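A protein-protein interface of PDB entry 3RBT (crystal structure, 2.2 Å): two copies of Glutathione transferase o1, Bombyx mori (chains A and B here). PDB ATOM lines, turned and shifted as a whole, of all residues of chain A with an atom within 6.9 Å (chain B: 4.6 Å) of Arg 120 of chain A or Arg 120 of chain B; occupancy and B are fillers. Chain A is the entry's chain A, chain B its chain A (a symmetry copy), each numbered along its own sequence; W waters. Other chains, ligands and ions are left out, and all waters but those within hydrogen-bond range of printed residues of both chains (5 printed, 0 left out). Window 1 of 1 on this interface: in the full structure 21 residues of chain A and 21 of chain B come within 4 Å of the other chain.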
ATOM      1  N   GLU A  91      13.004  14.398  31.333  1.00  0.00           N
ATOM      2  CA  GLU A  91      13.310  14.535  29.898  1.00  0.00           C
ATOM      3  C   GLU A  91      13.149  15.970  29.387  1.00  0.00           C
ATOM      4  O   GLU A  91      12.034  16.511  29.376  1.00  0.00           O
ATOM      5  CB  GLU A  91      12.516  13.531  29.049  1.00  0.00           C
ATOM      6  CG  GLU A  91      12.848  12.070  29.345  1.00  0.00           C
ATOM      7  CD  GLU A  91      12.339  11.116  28.286  1.00  0.00           C
ATOM      8  OE1 GLU A  91      12.027  11.577  27.164  1.00  0.00           O
ATOM      9  OE2 GLU A  91      12.253   9.889  28.573  1.00  0.00           O
ATOM     10  N   VAL A  93      13.097  17.725  26.629  1.00  0.00           N
ATOM     11  CA  VAL A  93      12.081  18.028  25.620  1.00  0.00           C
ATOM     12  C   VAL A  93      10.673  18.042  26.218  1.00  0.00           C
ATOM     13  O   VAL A  93       9.916  18.984  26.006  1.00  0.00           O
ATOM     14  CB  VAL A  93      12.124  17.028  24.438  1.00  0.00           C
ATOM     15  CG1 VAL A  93      11.037  17.375  23.414  1.00  0.00           C
ATOM     16  CG2 VAL A  93      13.501  17.045  23.778  1.00  0.00           C
ATOM     17  N   VAL A  94      10.329  16.997  26.964  1.00  0.00           N
ATOM     18  CA  VAL A  94       9.010  16.908  27.598  1.00  0.00           C
ATOM     19  C   VAL A  94       8.812  18.059  28.599  1.00  0.00           C
ATOM     20  O   VAL A  94       7.733  18.682  28.655  1.00  0.00           O
ATOM     21  CB  VAL A  94       8.817  15.538  28.276  1.00  0.00           C
ATOM     22  CG1 VAL A  94       7.499  15.476  29.021  1.00  0.00           C
ATOM     23  CG2 VAL A  94       8.886  14.430  27.233  1.00  0.00           C
ATOM     24  N   ILE A  95       9.874  18.346  29.351  1.00  0.00           N
ATOM     25  CA  ILE A  95       9.881  19.422  30.351  1.00  0.00           C
ATOM     26  C   ILE A  95       9.621  20.782  29.708  1.00  0.00           C
ATOM     27  O   ILE A  95       8.756  21.532  30.156  1.00  0.00           O
ATOM     28  CB  ILE A  95      11.209  19.453  31.151  1.00  0.00           C
ATOM     29  CG1 ILE A  95      11.239  18.295  32.167  1.00  0.00           C
ATOM     30  CG2 ILE A  95      11.351  20.762  31.879  1.00  0.00           C
ATOM     31  CD1 ILE A  95      12.643  17.960  32.743  1.00  0.00           C
ATOM     32  N   CYS A  96      10.360  21.080  28.644  1.00  0.00           N
ATOM     33  CA  CYS A  96      10.256  22.366  27.988  1.00  0.00           C
ATOM     34  C   CYS A  96       8.910  22.526  27.296  1.00  0.00           C
ATOM     35  O   CYS A  96       8.357  23.624  27.298  1.00  0.00           O
ATOM     36  CB  CYS A  96      11.404  22.559  26.990  1.00  0.00           C
ATOM     37  SG  CYS A  96      13.036  22.797  27.767  1.00  0.00           S
ATOM     38  N   ASP A  97       8.396  21.438  26.713  1.00  0.00           N
ATOM     39  CA  ASP A  97       7.084  21.448  26.062  1.00  0.00           C
ATOM     40  C   ASP A  97       5.954  21.599  27.081  1.00  0.00           C
ATOM     41  O   ASP A  97       4.988  22.333  26.836  1.00  0.00           O
ATOM     42  CB  ASP A  97       6.872  20.202  25.179  1.00  0.00           C
ATOM     43  CG  ASP A  97       7.736  20.228  23.904  1.00  0.00           C
ATOM     44  OD1 ASP A  97       8.329  21.281  23.586  1.00  0.00           O
ATOM     45  OD2 ASP A  97       7.804  19.199  23.206  1.00  0.00           O
ATOM     46  N   TYR A  98       6.103  20.931  28.226  1.00  0.00           N
ATOM     47  CA  TYR A  98       5.179  21.116  29.347  1.00  0.00           C
ATOM     48  C   TYR A  98       5.089  22.603  29.703  1.00  0.00           C
ATOM     49  O   TYR A  98       4.004  23.154  29.794  1.00  0.00           O
ATOM     50  CB  TYR A  98       5.607  20.304  30.584  1.00  0.00           C
ATOM     51  CG  TYR A  98       4.875  20.763  31.817  1.00  0.00           C
ATOM     52  CD1 TYR A  98       3.557  20.371  32.045  1.00  0.00           C
ATOM     53  CD2 TYR A  98       5.470  21.645  32.720  1.00  0.00           C
ATOM     54  CE1 TYR A  98       2.863  20.817  33.161  1.00  0.00           C
ATOM     55  CE2 TYR A  98       4.776  22.097  33.838  1.00  0.00           C
ATOM     56  CZ  TYR A  98       3.477  21.685  34.049  1.00  0.00           C
ATOM     57  OH  TYR A  98       2.776  22.131  35.155  1.00  0.00           O
ATOM     58  N   GLU A 101       3.256  24.790  27.097  1.00  0.00           N
ATOM     59  CA  GLU A 101       1.805  24.536  27.143  1.00  0.00           C
ATOM     60  C   GLU A 101       1.140  25.060  28.421  1.00  0.00           C
ATOM     61  O   GLU A 101       0.069  25.658  28.377  1.00  0.00           O
ATOM     62  CB  GLU A 101       1.540  23.028  27.063  1.00  0.00           C
ATOM     63  CG  GLU A 101       1.790  22.402  25.722  1.00  0.00           C
ATOM     64  CD  GLU A 101       1.622  20.890  25.710  1.00  0.00           C
ATOM     65  OE1 GLU A 101       1.910  20.290  24.662  1.00  0.00           O
ATOM     66  OE2 GLU A 101       1.221  20.283  26.725  1.00  0.00           O
ATOM     67  N   HIS A 109       7.003  27.704  20.931  1.00  0.00           N
ATOM     68  CA  HIS A 109       6.695  26.914  19.740  1.00  0.00           C
ATOM     69  C   HIS A 109       5.910  27.754  18.740  1.00  0.00           C
ATOM     70  O   HIS A 109       5.192  28.696  19.111  1.00  0.00           O
ATOM     71  CB  HIS A 109       5.896  25.646  20.082  1.00  0.00           C
ATOM     72  CG  HIS A 109       6.744  24.489  20.511  1.00  0.00           C
ATOM     73  ND1 HIS A 109       7.591  23.825  19.647  1.00  0.00           N
ATOM     74  CD2 HIS A 109       6.879  23.875  21.711  1.00  0.00           C
ATOM     75  CE1 HIS A 109       8.204  22.851  20.296  1.00  0.00           C
ATOM     76  NE2 HIS A 109       7.790  22.860  21.550  1.00  0.00           N
ATOM     77  N   TYR A 114       2.490  22.578  11.321  1.00  0.00           N
ATOM     78  CA  TYR A 114       3.504  22.100  10.375  1.00  0.00           C
ATOM     79  C   TYR A 114       4.908  22.586  10.753  1.00  0.00           C
ATOM     80  O   TYR A 114       5.851  21.781  10.828  1.00  0.00           O
ATOM     81  CB  TYR A 114       3.173  22.456   8.917  1.00  0.00           C
ATOM     82  CG  TYR A 114       4.291  22.086   7.953  1.00  0.00           C
ATOM     83  CD1 TYR A 114       4.714  20.760   7.822  1.00  0.00           C
ATOM     84  CD2 TYR A 114       4.938  23.059   7.192  1.00  0.00           C
ATOM     85  CE1 TYR A 114       5.737  20.411   6.952  1.00  0.00           C
ATOM     86  CE2 TYR A 114       5.976  22.718   6.319  1.00  0.00           C
ATOM     87  CZ  TYR A 114       6.368  21.389   6.213  1.00  0.00           C
ATOM     88  OH  TYR A 114       7.384  21.033   5.362  1.00  0.00           O
ATOM     89  N   VAL A 115       5.031  23.888  11.023  1.00  0.00           N
ATOM     90  CA  VAL A 115       6.311  24.487  11.415  1.00  0.00           C
ATOM     91  C   VAL A 115       6.807  23.866  12.729  1.00  0.00           C
ATOM     92  O   VAL A 115       7.989  23.569  12.882  1.00  0.00           O
ATOM     93  CB  VAL A 115       6.226  26.040  11.531  1.00  0.00           C
ATOM     94  CG1 VAL A 115       7.564  26.640  12.023  1.00  0.00           C
ATOM     95  CG2 VAL A 115       5.828  26.669  10.188  1.00  0.00           C
ATOM     96  N   LYS A 116       5.895  23.648  13.667  1.00  0.00           N
ATOM     97  CA  LYS A 116       6.264  23.040  14.941  1.00  0.00           C
ATOM     98  C   LYS A 116       6.751  21.596  14.728  1.00  0.00           C
ATOM     99  O   LYS A 116       7.752  21.192  15.306  1.00  0.00           O
ATOM    100  CB  LYS A 116       5.087  23.095  15.921  1.00  0.00           C
ATOM    101  CG  LYS A 116       5.306  22.295  17.213  1.00  0.00           C
ATOM    102  CD  LYS A 116       4.113  22.432  18.138  1.00  0.00           C
ATOM    103  CE  LYS A 116       4.338  21.656  19.431  1.00  0.00           C
ATOM    104  NZ  LYS A 116       3.154  21.875  20.292  1.00  0.00           N
ATOM    105  N   ALA A 117       6.045  20.833  13.895  1.00  0.00           N
ATOM    106  CA  ALA A 117       6.473  19.480  13.543  1.00  0.00           C
ATOM    107  C   ALA A 117       7.891  19.471  12.956  1.00  0.00           C
ATOM    108  O   ALA A 117       8.708  18.622  13.320  1.00  0.00           O
ATOM    109  CB  ALA A 117       5.479  18.833  12.586  1.00  0.00           C
ATOM    110  N   GLN A 118       8.181  20.427  12.072  1.00  0.00           N
ATOM    111  CA  GLN A 118       9.529  20.599  11.519  1.00  0.00           C
ATOM    112  C   GLN A 118      10.555  20.932  12.592  1.00  0.00           C
ATOM    113  O   GLN A 118      11.665  20.381  12.594  1.00  0.00           O
ATOM    114  CB  GLN A 118       9.560  21.670  10.416  1.00  0.00           C
ATOM    115  CG  GLN A 118       8.822  21.286   9.143  1.00  0.00           C
ATOM    116  CD  GLN A 118       9.176  19.886   8.648  1.00  0.00           C
ATOM    117  OE1 GLN A 118      10.321  19.607   8.285  1.00  0.00           O
ATOM    118  NE2 GLN A 118       8.185  19.002   8.630  1.00  0.00           N
ATOM    119  N   ASP A 119      10.176  21.820  13.504  1.00  0.00           N
ATOM    120  CA  ASP A 119      11.011  22.147  14.663  1.00  0.00           C
ATOM    121  C   ASP A 119      11.327  20.920  15.519  1.00  0.00           C
ATOM    122  O   ASP A 119      12.467  20.759  15.961  1.00  0.00           O
ATOM    123  CB  ASP A 119      10.359  23.245  15.517  1.00  0.00           C
ATOM    124  CG  ASP A 119      10.508  24.629  14.897  1.00  0.00           C
ATOM    125  OD1 ASP A 119      11.154  24.740  13.838  1.00  0.00           O
ATOM    126  OD2 ASP A 119       9.980  25.605  15.463  1.00  0.00           O
ATOM    127  N   ARG A 120      10.321  20.071  15.751  1.00  0.00           N
ATOM    128  CA  ARG A 120      10.515  18.829  16.509  1.00  0.00           C
ATOM    129  C   ARG A 120      11.448  17.861  15.795  1.00  0.00           C
ATOM    130  O   ARG A 120      12.260  17.202  16.440  1.00  0.00           O
ATOM    131  CB  ARG A 120       9.176  18.144  16.840  1.00  0.00           C
ATOM    132  CG  ARG A 120       8.322  18.917  17.850  1.00  0.00           C
ATOM    133  CD  ARG A 120       7.084  18.133  18.262  1.00  0.00           C
ATOM    134  NE  ARG A 120       7.419  16.907  18.988  1.00  0.00           N
ATOM    135  CZ  ARG A 120       6.534  15.985  19.361  1.00  0.00           C
ATOM    136  NH1 ARG A 120       5.250  16.127  19.069  1.00  0.00           N
ATOM    137  NH2 ARG A 120       6.935  14.915  20.027  1.00  0.00           N
ATOM    138  N   LEU A 121      11.329  17.784  14.471  1.00  0.00           N
ATOM    139  CA  LEU A 121      12.205  16.938  13.654  1.00  0.00           C
ATOM    140  C   LEU A 121      13.661  17.392  13.699  1.00  0.00           C
ATOM    141  O   LEU A 121      14.583  16.562  13.710  1.00  0.00           O
ATOM    142  CB  LEU A 121      11.701  16.863  12.208  1.00  0.00           C
ATOM    143  CG  LEU A 121      10.408  16.050  12.042  1.00  0.00           C
ATOM    144  CD1 LEU A 121       9.893  16.082  10.607  1.00  0.00           C
ATOM    145  CD2 LEU A 121      10.596  14.616  12.522  1.00  0.00           C
ATOM    146  N   LEU A 122      13.852  18.711  13.760  1.00  0.00           N
ATOM    147  CA  LEU A 122      15.178  19.317  13.830  1.00  0.00           C
ATOM    148  C   LEU A 122      15.821  19.106  15.203  1.00  0.00           C
ATOM    149  O   LEU A 122      17.022  18.834  15.294  1.00  0.00           O
ATOM    150  CB  LEU A 122      15.111  20.800  13.448  1.00  0.00           C
ATOM    151  CG  LEU A 122      14.840  21.009  11.948  1.00  0.00           C
ATOM    152  CD1 LEU A 122      14.246  22.381  11.653  1.00  0.00           C
ATOM    153  CD2 LEU A 122      16.097  20.758  11.099  1.00  0.00           C
ATOM    154  N   ILE A 123      15.021  19.205  16.263  1.00  0.00           N
ATOM    155  CA  ILE A 123      15.500  18.862  17.601  1.00  0.00           C
ATOM    156  C   ILE A 123      16.039  17.426  17.627  1.00  0.00           C
ATOM    157  O   ILE A 123      17.136  17.177  18.146  1.00  0.00           O
ATOM    158  CB  ILE A 123      14.433  19.093  18.707  1.00  0.00           C
ATOM    159  CG1 ILE A 123      14.119  20.595  18.828  1.00  0.00           C
ATOM    160  CG2 ILE A 123      14.944  18.566  20.045  1.00  0.00           C
ATOM    161  CD1 ILE A 123      12.767  20.918  19.484  1.00  0.00           C
ATOM    162  N   GLU A 124      15.278  16.490  17.053  1.00  0.00           N
ATOM    163  CA  GLU A 124      15.737  15.114  16.966  1.00  0.00           C
ATOM    164  C   GLU A 124      17.027  14.996  16.141  1.00  0.00           C
ATOM    165  O   GLU A 124      17.997  14.381  16.591  1.00  0.00           O
ATOM    166  CB  GLU A 124      14.632  14.209  16.425  1.00  0.00           C
ATOM    167  CG  GLU A 124      15.028  12.747  16.294  1.00  0.00           C
ATOM    168  CD  GLU A 124      15.202  12.028  17.629  1.00  0.00           C
ATOM    169  OE1 GLU A 124      15.825  10.939  17.622  1.00  0.00           O
ATOM    170  OE2 GLU A 124      14.715  12.525  18.672  1.00  0.00           O
ATOM    171  N   ARG A 125      17.032  15.582  14.942  1.00  0.00           N
ATOM    172  CA  ARG A 125      18.242  15.679  14.119  1.00  0.00           C
ATOM    173  C   ARG A 125      19.474  16.224  14.858  1.00  0.00           C
ATOM    174  O   ARG A 125      20.592  15.737  14.648  1.00  0.00           O
ATOM    175  CB  ARG A 125      17.982  16.541  12.881  1.00  0.00           C
ATOM    176  CG  ARG A 125      17.390  15.799  11.722  1.00  0.00           C
ATOM    177  CD  ARG A 125      16.777  16.768  10.726  1.00  0.00           C
ATOM    178  NE  ARG A 125      15.857  16.099   9.811  1.00  0.00           N
ATOM    179  CZ  ARG A 125      14.774  16.665   9.287  1.00  0.00           C
ATOM    180  NH1 ARG A 125      14.456  17.918   9.592  1.00  0.00           N
ATOM    181  NH2 ARG A 125      13.994  15.970   8.466  1.00  0.00           N
ATOM    182  N   LEU A 175      13.045  26.190  19.089  1.00  0.00           N
ATOM    183  CA  LEU A 175      14.191  25.533  18.443  1.00  0.00           C
ATOM    184  C   LEU A 175      15.528  26.231  18.787  1.00  0.00           C
ATOM    185  O   LEU A 175      16.492  25.571  19.182  1.00  0.00           O
ATOM    186  CB  LEU A 175      13.986  25.412  16.926  1.00  0.00           C
ATOM    187  CG  LEU A 175      15.078  24.692  16.121  1.00  0.00           C
ATOM    188  CD1 LEU A 175      15.291  23.232  16.603  1.00  0.00           C
ATOM    189  CD2 LEU A 175      14.775  24.731  14.627  1.00  0.00           C
ATOM    190  N   VAL B  93       5.532   9.645  16.108  1.00  0.00           N
ATOM    191  CA  VAL B  93       5.151  10.533  17.208  1.00  0.00           C
ATOM    192  C   VAL B  93       4.873  11.955  16.719  1.00  0.00           C
ATOM    193  O   VAL B  93       3.843  12.536  17.046  1.00  0.00           O
ATOM    194  CB  VAL B  93       6.230  10.576  18.317  1.00  0.00           C
ATOM    195  CG1 VAL B  93       5.795  11.526  19.440  1.00  0.00           C
ATOM    196  CG2 VAL B  93       6.477   9.175  18.873  1.00  0.00           C
ATOM    197  N   VAL B  94       5.793  12.509  15.935  1.00  0.00           N
ATOM    198  CA  VAL B  94       5.628  13.863  15.397  1.00  0.00           C
ATOM    199  C   VAL B  94       4.389  13.937  14.489  1.00  0.00           C
ATOM    200  O   VAL B  94       3.603  14.903  14.553  1.00  0.00           O
ATOM    201  CB  VAL B  94       6.897  14.316  14.649  1.00  0.00           C
ATOM    202  CG1 VAL B  94       6.697  15.672  14.002  1.00  0.00           C
ATOM    203  CG2 VAL B  94       8.077  14.360  15.612  1.00  0.00           C
ATOM    204  N   ASP B  97       1.137  13.684  16.611  1.00  0.00           N
ATOM    205  CA  ASP B  97       0.971  14.934  17.358  1.00  0.00           C
ATOM    206  C   ASP B  97       0.570  16.088  16.437  1.00  0.00           C
ATOM    207  O   ASP B  97      -0.285  16.905  16.800  1.00  0.00           O
ATOM    208  CB  ASP B  97       2.231  15.286  18.173  1.00  0.00           C
ATOM    209  CG  ASP B  97       2.434  14.351  19.379  1.00  0.00           C
ATOM    210  OD1 ASP B  97       1.514  13.577  19.718  1.00  0.00           O
ATOM    211  OD2 ASP B  97       3.511  14.405  20.003  1.00  0.00           O
ATOM    212  N   LYS B 116      -0.458  14.965  29.921  1.00  0.00           N
ATOM    213  CA  LYS B 116       0.104  14.780  28.587  1.00  0.00           C
ATOM    214  C   LYS B 116       1.618  14.518  28.671  1.00  0.00           C
ATOM    215  O   LYS B 116       2.129  13.633  27.996  1.00  0.00           O
ATOM    216  CB  LYS B 116      -0.207  15.992  27.703  1.00  0.00           C
ATOM    217  CG  LYS B 116       0.519  15.988  26.350  1.00  0.00           C
ATOM    218  CD  LYS B 116       0.129  17.199  25.528  1.00  0.00           C
ATOM    219  CE  LYS B 116       0.833  17.184  24.174  1.00  0.00           C
ATOM    220  NZ  LYS B 116       0.369  18.370  23.420  1.00  0.00           N
ATOM    221  N   ALA B 117       2.322  15.283  29.504  1.00  0.00           N
ATOM    222  CA  ALA B 117       3.747  15.057  29.737  1.00  0.00           C
ATOM    223  C   ALA B 117       4.020  13.624  30.215  1.00  0.00           C
ATOM    224  O   ALA B 117       4.957  12.978  29.738  1.00  0.00           O
ATOM    225  CB  ALA B 117       4.301  16.078  30.722  1.00  0.00           C
ATOM    226  N   GLN B 118       3.190  13.128  31.133  1.00  0.00           N
ATOM    227  CA  GLN B 118       3.271  11.738  31.595  1.00  0.00           C
ATOM    228  C   GLN B 118       3.023  10.742  30.472  1.00  0.00           C
ATOM    229  O   GLN B 118       3.739   9.737  30.352  1.00  0.00           O
ATOM    230  CB  GLN B 118       2.303  11.465  32.758  1.00  0.00           C
ATOM    231  CG  GLN B 118       2.662  12.174  34.056  1.00  0.00           C
ATOM    232  CD  GLN B 118       4.132  12.018  34.432  1.00  0.00           C
ATOM    233  OE1 GLN B 118       4.613  10.911  34.691  1.00  0.00           O
ATOM    234  NE2 GLN B 118       4.851  13.135  34.469  1.00  0.00           N
ATOM    235  N   ASP B 119       2.022  11.031  29.648  1.00  0.00           N
ATOM    236  CA  ASP B 119       1.743  10.229  28.454  1.00  0.00           C
ATOM    237  C   ASP B 119       2.937  10.170  27.500  1.00  0.00           C
ATOM    238  O   ASP B 119       3.241   9.100  26.965  1.00  0.00           O
ATOM    239  CB  ASP B 119       0.497  10.750  27.722  1.00  0.00           C
ATOM    240  CG  ASP B 119      -0.797  10.342  28.416  1.00  0.00           C
ATOM    241  OD1 ASP B 119      -0.727   9.620  29.429  1.00  0.00           O
ATOM    242  OD2 ASP B 119      -1.883  10.741  27.954  1.00  0.00           O
ATOM    243  N   ARG B 120       3.599  11.311  27.290  1.00  0.00           N
ATOM    244  CA  ARG B 120       4.797  11.368  26.443  1.00  0.00           C
ATOM    245  C   ARG B 120       5.949  10.560  27.022  1.00  0.00           C
ATOM    246  O   ARG B 120       6.676   9.906  26.278  1.00  0.00           O
ATOM    247  CB  ARG B 120       5.238  12.818  26.170  1.00  0.00           C
ATOM    248  CG  ARG B 120       4.269  13.600  25.277  1.00  0.00           C
ATOM    249  CD  ARG B 120       4.817  14.970  24.909  1.00  0.00           C
ATOM    250  NE  ARG B 120       6.023  14.884  24.084  1.00  0.00           N
ATOM    251  CZ  ARG B 120       6.765  15.927  23.720  1.00  0.00           C
ATOM    252  NH1 ARG B 120       6.447  17.150  24.116  1.00  0.00           N
ATOM    253  NH2 ARG B 120       7.833  15.746  22.959  1.00  0.00           N
ATOM    254  N   LEU B 121       6.105  10.604  28.344  1.00  0.00           N
ATOM    255  CA  LEU B 121       7.136   9.826  29.037  1.00  0.00           C
ATOM    256  C   LEU B 121       6.912   8.322  28.914  1.00  0.00           C
ATOM    257  O   LEU B 121       7.872   7.548  28.781  1.00  0.00           O
ATOM    258  CB  LEU B 121       7.238  10.242  30.510  1.00  0.00           C
ATOM    259  CG  LEU B 121       7.850  11.636  30.720  1.00  0.00           C
ATOM    260  CD1 LEU B 121       7.845  12.047  32.188  1.00  0.00           C
ATOM    261  CD2 LEU B 121       9.256  11.712  30.137  1.00  0.00           C
ATOM    262  N   LEU B 122       5.637   7.925  28.922  1.00  0.00           N
ATOM    263  CA  LEU B 122       5.242   6.527  28.792  1.00  0.00           C
ATOM    264  C   LEU B 122       5.448   6.015  27.365  1.00  0.00           C
ATOM    265  O   LEU B 122       5.896   4.880  27.167  1.00  0.00           O
ATOM    266  CB  LEU B 122       3.799   6.330  29.272  1.00  0.00           C
ATOM    267  CG  LEU B 122       3.663   6.468  30.798  1.00  0.00           C
ATOM    268  CD1 LEU B 122       2.241   6.814  31.223  1.00  0.00           C
ATOM    269  CD2 LEU B 122       4.170   5.217  31.533  1.00  0.00           C
ATOM    270  N   ILE B 123       5.147   6.854  26.375  1.00  0.00           N
ATOM    271  CA  ILE B 123       5.459   6.522  24.987  1.00  0.00           C
ATOM    272  C   ILE B 123       6.956   6.223  24.830  1.00  0.00           C
ATOM    273  O   ILE B 123       7.333   5.216  24.215  1.00  0.00           O
ATOM    274  CB  ILE B 123       4.983   7.606  23.980  1.00  0.00           C
ATOM    275  CG1 ILE B 123       3.446   7.681  23.978  1.00  0.00           C
ATOM    276  CG2 ILE B 123       5.482   7.272  22.577  1.00  0.00           C
ATOM    277  CD1 ILE B 123       2.868   9.003  23.446  1.00  0.00           C
ATOM    278  N   GLU B 124       7.802   7.087  25.398  1.00  0.00           N
ATOM    279  CA  GLU B 124       9.235   6.850  25.363  1.00  0.00           C
ATOM    280  C   GLU B 124       9.614   5.546  26.080  1.00  0.00           C
ATOM    281  O   GLU B 124      10.337   4.718  25.521  1.00  0.00           O
ATOM    282  CB  GLU B 124       9.995   8.049  25.926  1.00  0.00           C
ATOM    283  CG  GLU B 124      11.507   7.885  25.934  1.00  0.00           C
ATOM    284  CD  GLU B 124      12.142   7.915  24.547  1.00  0.00           C
ATOM    285  OE1 GLU B 124      13.313   7.475  24.438  1.00  0.00           O
ATOM    286  OE2 GLU B 124      11.499   8.380  23.576  1.00  0.00           O
HETATM  287  O   HOH W   1       3.728  16.826  21.890  1.00  0.00           O
HETATM  288  O   HOH W   2       6.173  12.812  22.362  1.00  0.00           O
HETATM  289  O   HOH W   3      10.360   8.092  29.757  1.00  0.00           O
HETATM  290  O   HOH W   4       5.312  18.716  21.466  1.00  0.00           O
HETATM  291  O   HOH W   5       9.611  16.982  20.559  1.00  0.00           O
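The guanidinium group (NH1) of Arg 120 of chain B lies within salt-bridge range of the side-chain carboxylate (OD2) of Asp 97 of chain A. The guanidinium group (NH2) of Arg 120 of chain B sits close to the guanidinium group (NH2) of Arg 120 of chain A, 3.2 Å away. NH1 of Arg 120 of chain A is in salt-bridge range of OD2 of Asp 97 of chain B (2.6 Å). The side-chain amino group of Lys 116 of chain B lies within salt-bridge range of the side-chain carboxylate of Glu 101 of chain A, 2.8 Å away.
OD1 of Asp 97 of chain A sits at hydrogen-bond distance from NE2 of His 109 of chain A.
Among the printed residues, pairs that only touch across the chains: Glu 91 of chain A with Leu 121 of chain B (3.6 Å), Glu 91 of chain A with Glu 124 of chain B (3.4 Å), Val 93 of chain A with Arg 120 of chain B (3.6 Å), Val 94 of chain A with Ala 117 of chain B (3.6 Å), Val 94 of chain A with Leu 121 of chain B (3.99 Å), Ala 117 of chain A with Val 94 of chain B (3.6 Å), Arg 120 of chain A with Val 93 of chain B (3.6 Å) and Leu 121 of chain A with Val 94 of chain B (3.99 Å).
Of the printed residues of chain B, Val 93 of chain A touches Arg 120 (3.6 Å). His 109 of chain A touches none of the printed residues of chain B. Arg 120 of chain A touches three residues of chain B. Of the printed residues of chain B, Leu 121 of chain A touches Val 94 (3.99 Å). Arg 120 of chain B touches three residues of chain A. Ile 123 of chain B touches none of the printed residues of chain A. The nearest residue of chain B that does not touch Arg 120 of chain A is Val 94 of chain B (4.1 Å). The nearest residue of chain A that does not touch Arg 120 of chain B is Val 94 of chain A (4.1 Å). The nearest printed residue of chain B that does not touch Ala 117 of chain A is Asp 97 of chain B (6.8 Å).
Of the 12 printed residues of chain B, 8 touch a printed residue of chain A. Hydrophobic or aromatic side chains of chain B within 4 Å of the printed part of chain A: Val 93, Val 94, Ala 117 and Leu 121. Printed residues of chain A that touch a printed residue of chain B: Glu 91, Val 93, Val 94, Asp 97, Glu 101, Ala 117, Arg 120 and Leu 121. Hydrophobic or aromatic side chains of chain A within 4 Å of the printed part of chain B: Val 93, Val 94, Ala 117 and Leu 121.
Val 93 of chain A touches Arg 120 of chain B, and with the chains exchanged Arg 120 of chain A touches Val 93 of chain B. Val 94 of chain A touches Ala 117 of chain B, and with the chains exchanged Ala 117 of chain A touches Val 94 of chain B. Asp 97 of chain A touches Arg 120 of chain B, and with the chains exchanged Arg 120 of chain A touches Asp 97 of chain B. Arg 120 of chain A touches its own counterpart, Arg 120 of chain B. Of the 12 pairs that touch across the chains among the printed residues, 9 have their exchanged pair printed and touching as well.
Water W5 lies within hydrogen-bond range of the guanidinium group of Arg 120 of chain A (2.7 Å) and the guanidinium group of Arg 120 of chain B (3.2 Å). Water W2 bridges the guanidinium group (NE) of Arg 120 of chain B and the guanidinium group (NH2) of Arg 120 of chain A. Water W3 lies within hydrogen-bond range of O of Leu 121 of chain B and OE2 of Glu 91 of chain A. Water W4 bridges OD2 of Asp 97 of chain A and NH1 of Arg 120 of chain B. Water W1 bridges the side-chain carboxylate of Asp 97 of chain B (3.1 Å) and the guanidinium group of Arg 120 of chain A (3.3 Å).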
